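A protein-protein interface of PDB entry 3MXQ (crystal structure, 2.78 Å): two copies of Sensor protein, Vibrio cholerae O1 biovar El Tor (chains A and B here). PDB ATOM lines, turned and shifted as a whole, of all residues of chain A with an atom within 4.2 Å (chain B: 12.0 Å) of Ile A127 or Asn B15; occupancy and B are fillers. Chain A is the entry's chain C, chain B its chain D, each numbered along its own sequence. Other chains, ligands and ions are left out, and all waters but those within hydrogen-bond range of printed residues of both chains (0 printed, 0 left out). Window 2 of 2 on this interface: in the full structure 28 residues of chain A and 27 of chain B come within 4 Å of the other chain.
The backbone NH (N) of His A128 lies within hydrogen-bond range of the side-chain amide oxygen (OD1) of Asn B15, at 2.8 Å.
The backbone carbonyl oxygen (O) of Ile A127 is in hydrogen-bond range of the backbone NH (N) of Glu A135. O of His A136 lies within hydrogen-bond range of N of Ile A127, 2.8 Å away.
Ser B14 touches Ile A125. Ile A125 touches Met B17 (CG2 to CB, 3.9 Å). Ile A125 touches Ala B18. CD1 of Ile A125 touches CG of Arg B21, 3.7 Å away. Pro A126 touches Ser B14. OD1 of Asn B15 touches CA of Ile A127, at 3.7 Å. Ile A127 touches Ala B18. His A128 touches Phe B12 (CG to CD1, 3.6 Å).
Pro A126 touches just one residue of chain B: Ser B14. Ile A134 touches none of the printed residues of chain B. No residue of chain B comes within 4 Å of Glu A135. No residue of chain B comes within 4 Å of His A136. Printed residues of chain A within 4 Å of Arg B21: Ile A125 (3.7 Å). Printed residues of chain A within 4 Å of Phe B12: His A128 (3.6 Å). Ser B25 touches none of the printed residues of chain A. Leu B10 touches none of the printed residues of chain A. The nearest residue of chain B that does not touch Ile A127 is Leu B22 (5.2 Å). The nearest residue of chain A that does not touch Asn B15 is Pro A126 (4.04 Å).
Of the 16 printed residues of chain B, 6 touch a printed residue of chain A. Hydrophobic or aromatic side chains of chain B that line the printed part of chain A: Phe B12, Met B17 and Ala B18. Of the 9 printed residues of chain A, 4 touch a printed residue of chain B. Printed residues of chain A that touch a printed residue of chain B: Ile A125, Pro A126, Ile A127 and His A128.
No position is printed for both chains.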
ATOM      1  N   ILE A 125      17.818  -6.738  22.853  1.00  0.00           N
ATOM      2  CA  ILE A 125      17.783  -7.408  21.544  1.00  0.00           C
ATOM      3  C   ILE A 125      18.763  -8.590  21.521  1.00  0.00           C
ATOM      4  O   ILE A 125      19.959  -8.430  21.787  1.00  0.00           O
ATOM      5  CB  ILE A 125      18.152  -6.434  20.386  1.00  0.00           C
ATOM      6  CG1 ILE A 125      17.329  -5.145  20.459  1.00  0.00           C
ATOM      7  CG2 ILE A 125      17.946  -7.084  19.045  1.00  0.00           C
ATOM      8  CD1 ILE A 125      18.031  -3.925  19.870  1.00  0.00           C
ATOM      9  N   PRO A 126      18.258  -9.788  21.213  1.00  0.00           N
ATOM     10  CA  PRO A 126      19.078 -10.980  21.074  1.00  0.00           C
ATOM     11  C   PRO A 126      19.910 -10.956  19.793  1.00  0.00           C
ATOM     12  O   PRO A 126      19.388 -10.597  18.742  1.00  0.00           O
ATOM     13  CB  PRO A 126      18.035 -12.095  20.953  1.00  0.00           C
ATOM     14  CG  PRO A 126      16.795 -11.527  21.479  1.00  0.00           C
ATOM     15  CD  PRO A 126      16.833 -10.105  21.092  1.00  0.00           C
ATOM     16  N   ILE A 127      21.182 -11.343  19.865  1.00  0.00           N
ATOM     17  CA  ILE A 127      21.969 -11.546  18.644  1.00  0.00           C
ATOM     18  C   ILE A 127      22.248 -13.028  18.405  1.00  0.00           C
ATOM     19  O   ILE A 127      22.909 -13.682  19.220  1.00  0.00           O
ATOM     20  CB  ILE A 127      23.292 -10.773  18.662  1.00  0.00           C
ATOM     21  CG1 ILE A 127      23.027  -9.282  18.891  1.00  0.00           C
ATOM     22  CG2 ILE A 127      24.032 -11.003  17.351  1.00  0.00           C
ATOM     23  CD1 ILE A 127      24.261  -8.429  19.107  1.00  0.00           C
ATOM     24  N   HIS A 128      21.757 -13.537  17.275  1.00  0.00           N
ATOM     25  CA  HIS A 128      21.860 -14.960  16.933  1.00  0.00           C
ATOM     26  C   HIS A 128      23.158 -15.301  16.227  1.00  0.00           C
ATOM     27  O   HIS A 128      23.575 -14.600  15.315  1.00  0.00           O
ATOM     28  CB  HIS A 128      20.701 -15.377  16.040  1.00  0.00           C
ATOM     29  CG  HIS A 128      19.355 -15.264  16.689  1.00  0.00           C
ATOM     30  ND1 HIS A 128      18.712 -16.340  17.262  1.00  0.00           N
ATOM     31  CD2 HIS A 128      18.522 -14.207  16.837  1.00  0.00           C
ATOM     32  CE1 HIS A 128      17.543 -15.950  17.736  1.00  0.00           C
ATOM     33  NE2 HIS A 128      17.404 -14.659  17.495  1.00  0.00           N
ATOM     34  N   SER A 129      23.785 -16.391  16.654  1.00  0.00           N
ATOM     35  CA  SER A 129      24.973 -16.925  15.989  1.00  0.00           C
ATOM     36  C   SER A 129      24.652 -17.589  14.652  1.00  0.00           C
ATOM     37  O   SER A 129      23.493 -17.863  14.341  1.00  0.00           O
ATOM     38  CB  SER A 129      25.686 -17.945  16.884  1.00  0.00           C
ATOM     39  OG  SER A 129      26.740 -17.349  17.620  1.00  0.00           O
ATOM     40  N   THR A 133      21.963 -19.950  17.794  1.00  0.00           N
ATOM     41  CA  THR A 133      21.845 -19.663  19.224  1.00  0.00           C
ATOM     42  C   THR A 133      22.222 -18.228  19.568  1.00  0.00           C
ATOM     43  O   THR A 133      23.083 -17.631  18.929  1.00  0.00           O
ATOM     44  CB  THR A 133      22.729 -20.611  20.065  1.00  0.00           C
ATOM     45  OG1 THR A 133      24.091 -20.507  19.629  1.00  0.00           O
ATOM     46  CG2 THR A 133      22.254 -22.070  19.933  1.00  0.00           C
ATOM     47  N   ILE A 134      21.569 -17.685  20.589  1.00  0.00           N
ATOM     48  CA  ILE A 134      21.859 -16.351  21.093  1.00  0.00           C
ATOM     49  C   ILE A 134      23.165 -16.379  21.871  1.00  0.00           C
ATOM     50  O   ILE A 134      23.259 -17.048  22.888  1.00  0.00           O
ATOM     51  CB  ILE A 134      20.778 -15.878  22.072  1.00  0.00           C
ATOM     52  CG1 ILE A 134      19.369 -16.231  21.583  1.00  0.00           C
ATOM     53  CG2 ILE A 134      20.925 -14.398  22.363  1.00  0.00           C
ATOM     54  CD1 ILE A 134      18.964 -15.605  20.310  1.00  0.00           C
ATOM     55  N   GLU A 135      24.168 -15.647  21.411  1.00  0.00           N
ATOM     56  CA  GLU A 135      25.455 -15.655  22.092  1.00  0.00           C
ATOM     57  C   GLU A 135      25.834 -14.283  22.617  1.00  0.00           C
ATOM     58  O   GLU A 135      26.722 -14.147  23.460  1.00  0.00           O
ATOM     59  CB  GLU A 135      26.548 -16.217  21.185  1.00  0.00           C
ATOM     60  CG  GLU A 135      26.524 -17.741  21.090  1.00  0.00           C
ATOM     61  CD  GLU A 135      27.829 -18.328  20.574  1.00  0.00           C
ATOM     62  OE1 GLU A 135      28.659 -17.568  20.017  1.00  0.00           O
ATOM     63  OE2 GLU A 135      28.019 -19.557  20.722  1.00  0.00           O
ATOM     64  N   HIS A 136      25.164 -13.269  22.092  1.00  0.00           N
ATOM     65  CA  HIS A 136      25.263 -11.920  22.618  1.00  0.00           C
ATOM     66  C   HIS A 136      23.861 -11.355  22.696  1.00  0.00           C
ATOM     67  O   HIS A 136      22.955 -11.787  21.972  1.00  0.00           O
ATOM     68  CB  HIS A 136      26.123 -11.029  21.718  1.00  0.00           C
ATOM     69  CG  HIS A 136      27.538 -11.491  21.581  1.00  0.00           C
ATOM     70  ND1 HIS A 136      27.889 -12.613  20.865  1.00  0.00           N
ATOM     71  CD2 HIS A 136      28.696 -10.968  22.048  1.00  0.00           C
ATOM     72  CE1 HIS A 136      29.201 -12.768  20.902  1.00  0.00           C
ATOM     73  NE2 HIS A 136      29.715 -11.781  21.612  1.00  0.00           N
ATOM     74  N   LEU B  10      22.256 -12.318   9.985  1.00  0.00           N
ATOM     75  CA  LEU B  10      21.347 -11.177   9.648  1.00  0.00           C
ATOM     76  C   LEU B  10      19.971 -11.613   9.104  1.00  0.00           C
ATOM     77  O   LEU B  10      19.134 -10.762   8.760  1.00  0.00           O
ATOM     78  CB  LEU B  10      22.034 -10.215   8.666  1.00  0.00           C
ATOM     79  CG  LEU B  10      21.899  -8.720   8.988  1.00  0.00           C
ATOM     80  CD1 LEU B  10      22.872  -8.320  10.101  1.00  0.00           C
ATOM     81  CD2 LEU B  10      22.120  -7.844   7.759  1.00  0.00           C
ATOM     82  N   TYR B  11      19.748 -12.929   9.031  1.00  0.00           N
ATOM     83  CA  TYR B  11      18.465 -13.505   8.578  1.00  0.00           C
ATOM     84  C   TYR B  11      17.337 -13.308   9.610  1.00  0.00           C
ATOM     85  O   TYR B  11      16.157 -13.241   9.243  1.00  0.00           O
ATOM     86  CB  TYR B  11      18.631 -15.003   8.223  1.00  0.00           C
ATOM     87  N   PHE B  12      17.716 -13.215  10.886  1.00  0.00           N
ATOM     88  CA  PHE B  12      16.785 -12.986  11.987  1.00  0.00           C
ATOM     89  C   PHE B  12      16.534 -11.502  12.135  1.00  0.00           C
ATOM     90  O   PHE B  12      17.455 -10.701  11.991  1.00  0.00           O
ATOM     91  CB  PHE B  12      17.374 -13.504  13.294  1.00  0.00           C
ATOM     92  CG  PHE B  12      17.947 -14.892  13.202  1.00  0.00           C
ATOM     93  CD1 PHE B  12      17.284 -15.970  13.794  1.00  0.00           C
ATOM     94  CD2 PHE B  12      19.155 -15.123  12.531  1.00  0.00           C
ATOM     95  CE1 PHE B  12      17.810 -17.263  13.716  1.00  0.00           C
ATOM     96  CE2 PHE B  12      19.688 -16.409  12.442  1.00  0.00           C
ATOM     97  CZ  PHE B  12      19.013 -17.484  13.039  1.00  0.00           C
ATOM     98  N   GLN B  13      15.296 -11.132  12.436  1.00  0.00           N
ATOM     99  CA  GLN B  13      14.953  -9.724  12.575  1.00  0.00           C
ATOM    100  C   GLN B  13      15.657  -9.091  13.778  1.00  0.00           C
ATOM    101  O   GLN B  13      16.026  -7.920  13.729  1.00  0.00           O
ATOM    102  CB  GLN B  13      13.436  -9.513  12.614  1.00  0.00           C
ATOM    103  CG  GLN B  13      12.842  -9.321  14.008  1.00  0.00           C
ATOM    104  CD  GLN B  13      11.331  -9.130  13.995  1.00  0.00           C
ATOM    105  OE1 GLN B  13      10.769  -8.577  13.047  1.00  0.00           O
ATOM    106  NE2 GLN B  13      10.666  -9.583  15.056  1.00  0.00           N
ATOM    107  N   SER B  14      15.864  -9.868  14.841  1.00  0.00           N
ATOM    108  CA  SER B  14      16.635  -9.408  15.995  1.00  0.00           C
ATOM    109  C   SER B  14      18.020  -8.922  15.565  1.00  0.00           C
ATOM    110  O   SER B  14      18.447  -7.845  15.963  1.00  0.00           O
ATOM    111  CB  SER B  14      16.736 -10.487  17.060  1.00  0.00           C
ATOM    112  N   ASN B  15      18.714  -9.688  14.731  1.00  0.00           N
ATOM    113  CA  ASN B  15      20.027  -9.264  14.262  1.00  0.00           C
ATOM    114  C   ASN B  15      19.964  -7.926  13.533  1.00  0.00           C
ATOM    115  O   ASN B  15      20.770  -7.033  13.808  1.00  0.00           O
ATOM    116  CB  ASN B  15      20.696 -10.335  13.397  1.00  0.00           C
ATOM    117  CG  ASN B  15      21.320 -11.463  14.225  1.00  0.00           C
ATOM    118  OD1 ASN B  15      20.721 -11.959  15.184  1.00  0.00           O
ATOM    119  ND2 ASN B  15      22.519 -11.881  13.843  1.00  0.00           N
ATOM    120  N   ALA B  16      18.993  -7.784  12.630  1.00  0.00           N
ATOM    121  CA  ALA B  16      18.761  -6.534  11.900  1.00  0.00           C
ATOM    122  C   ALA B  16      18.614  -5.377  12.869  1.00  0.00           C
ATOM    123  O   ALA B  16      19.182  -4.302  12.683  1.00  0.00           O
ATOM    124  CB  ALA B  16      17.519  -6.648  11.045  1.00  0.00           C
ATOM    125  N   MET B  17      17.840  -5.620  13.914  1.00  0.00           N
ATOM    126  CA  MET B  17      17.529  -4.629  14.910  1.00  0.00           C
ATOM    127  C   MET B  17      18.798  -4.163  15.613  1.00  0.00           C
ATOM    128  O   MET B  17      19.073  -2.962  15.710  1.00  0.00           O
ATOM    129  CB  MET B  17      16.597  -5.273  15.906  1.00  0.00           C
ATOM    130  CG  MET B  17      15.564  -4.373  16.451  1.00  0.00           C
ATOM    131  SD  MET B  17      14.097  -5.526  16.951  1.00  0.00           S
ATOM    132  CE  MET B  17      12.748  -4.092  17.056  1.00  0.00           C
ATOM    133  N   ALA B  18      19.563  -5.129  16.109  1.00  0.00           N
ATOM    134  CA  ALA B  18      20.858  -4.869  16.683  1.00  0.00           C
ATOM    135  C   ALA B  18      21.730  -4.054  15.718  1.00  0.00           C
ATOM    136  O   ALA B  18      22.261  -3.005  16.097  1.00  0.00           O
ATOM    137  CB  ALA B  18      21.528  -6.170  17.064  1.00  0.00           C
ATOM    138  N   LYS B  19      21.867  -4.515  14.475  1.00  0.00           N
ATOM    139  CA  LYS B  19      22.685  -3.795  13.490  1.00  0.00           C
ATOM    140  C   LYS B  19      22.336  -2.319  13.482  1.00  0.00           C
ATOM    141  O   LYS B  19      23.209  -1.471  13.692  1.00  0.00           O
ATOM    142  CB  LYS B  19      22.506  -4.368  12.081  1.00  0.00           C
ATOM    143  CG  LYS B  19      23.498  -3.832  11.058  1.00  0.00           C
ATOM    144  CD  LYS B  19      24.856  -4.499  11.224  1.00  0.00           C
ATOM    145  CE  LYS B  19      25.728  -4.325   9.980  1.00  0.00           C
ATOM    146  NZ  LYS B  19      26.621  -5.512   9.768  1.00  0.00           N
ATOM    147  N   SER B  20      21.056  -2.020  13.270  1.00  0.00           N
ATOM    148  CA  SER B  20      20.581  -0.642  13.288  1.00  0.00           C
ATOM    149  C   SER B  20      21.098   0.107  14.490  1.00  0.00           C
ATOM    150  O   SER B  20      21.739   1.144  14.330  1.00  0.00           O
ATOM    151  CB  SER B  20      19.065  -0.575  13.283  1.00  0.00           C
ATOM    152  OG  SER B  20      18.575  -0.965  12.015  1.00  0.00           O
ATOM    153  N   ARG B  21      20.834  -0.431  15.684  1.00  0.00           N
ATOM    154  CA  ARG B  21      21.192   0.246  16.922  1.00  0.00           C
ATOM    155  C   ARG B  21      22.682   0.506  16.914  1.00  0.00           C
ATOM    156  O   ARG B  21      23.107   1.618  17.207  1.00  0.00           O
ATOM    157  CB  ARG B  21      20.811  -0.566  18.149  1.00  0.00           C
ATOM    158  CG  ARG B  21      19.305  -0.754  18.438  1.00  0.00           C
ATOM    159  CD  ARG B  21      18.447   0.531  18.468  1.00  0.00           C
ATOM    160  NE  ARG B  21      17.692   0.636  17.213  1.00  0.00           N
ATOM    161  CZ  ARG B  21      16.519   0.038  16.966  1.00  0.00           C
ATOM    162  NH1 ARG B  21      15.912  -0.686  17.904  1.00  0.00           N
ATOM    163  NH2 ARG B  21      15.936   0.187  15.777  1.00  0.00           N
ATOM    164  N   LEU B  22      23.467  -0.500  16.531  1.00  0.00           N
ATOM    165  CA  LEU B  22      24.912  -0.334  16.423  1.00  0.00           C
ATOM    166  C   LEU B  22      25.347   0.768  15.442  1.00  0.00           C
ATOM    167  O   LEU B  22      26.173   1.639  15.792  1.00  0.00           O
ATOM    168  CB  LEU B  22      25.594  -1.658  16.086  1.00  0.00           C
ATOM    169  CG  LEU B  22      25.683  -2.634  17.251  1.00  0.00           C
ATOM    170  CD1 LEU B  22      25.899  -4.054  16.756  1.00  0.00           C
ATOM    171  CD2 LEU B  22      26.769  -2.208  18.218  1.00  0.00           C
ATOM    172  N   LEU B  23      24.781   0.743  14.234  1.00  0.00           N
ATOM    173  CA  LEU B  23      25.065   1.772  13.223  1.00  0.00           C
ATOM    174  C   LEU B  23      24.721   3.188  13.696  1.00  0.00           C
ATOM    175  O   LEU B  23      25.512   4.131  13.502  1.00  0.00           O
ATOM    176  CB  LEU B  23      24.327   1.464  11.923  1.00  0.00           C
ATOM    177  CG  LEU B  23      24.828   0.271  11.102  1.00  0.00           C
ATOM    178  CD1 LEU B  23      24.071   0.198   9.808  1.00  0.00           C
ATOM    179  CD2 LEU B  23      26.331   0.371  10.815  1.00  0.00           C
ATOM    180  N   LEU B  24      23.550   3.336  14.323  1.00  0.00           N
ATOM    181  CA  LEU B  24      23.126   4.633  14.841  1.00  0.00           C
ATOM    182  C   LEU B  24      24.093   5.109  15.904  1.00  0.00           C
ATOM    183  O   LEU B  24      24.404   6.292  16.001  1.00  0.00           O
ATOM    184  CB  LEU B  24      21.721   4.568  15.429  1.00  0.00           C
ATOM    185  CG  LEU B  24      21.228   5.926  15.950  1.00  0.00           C
ATOM    186  CD1 LEU B  24      21.239   6.991  14.853  1.00  0.00           C
ATOM    187  CD2 LEU B  24      19.859   5.832  16.610  1.00  0.00           C
ATOM    188  N   SER B  25      24.574   4.168  16.700  1.00  0.00           N
ATOM    189  CA  SER B  25      25.493   4.498  17.753  1.00  0.00           C
ATOM    190  C   SER B  25      26.809   5.008  17.141  1.00  0.00           C
ATOM    191  O   SER B  25      27.458   5.898  17.707  1.00  0.00           O
ATOM    192  CB  SER B  25      25.719   3.282  18.650  1.00  0.00           C
ATOM    193  OG  SER B  25      26.674   3.561  19.661  1.00  0.00           O
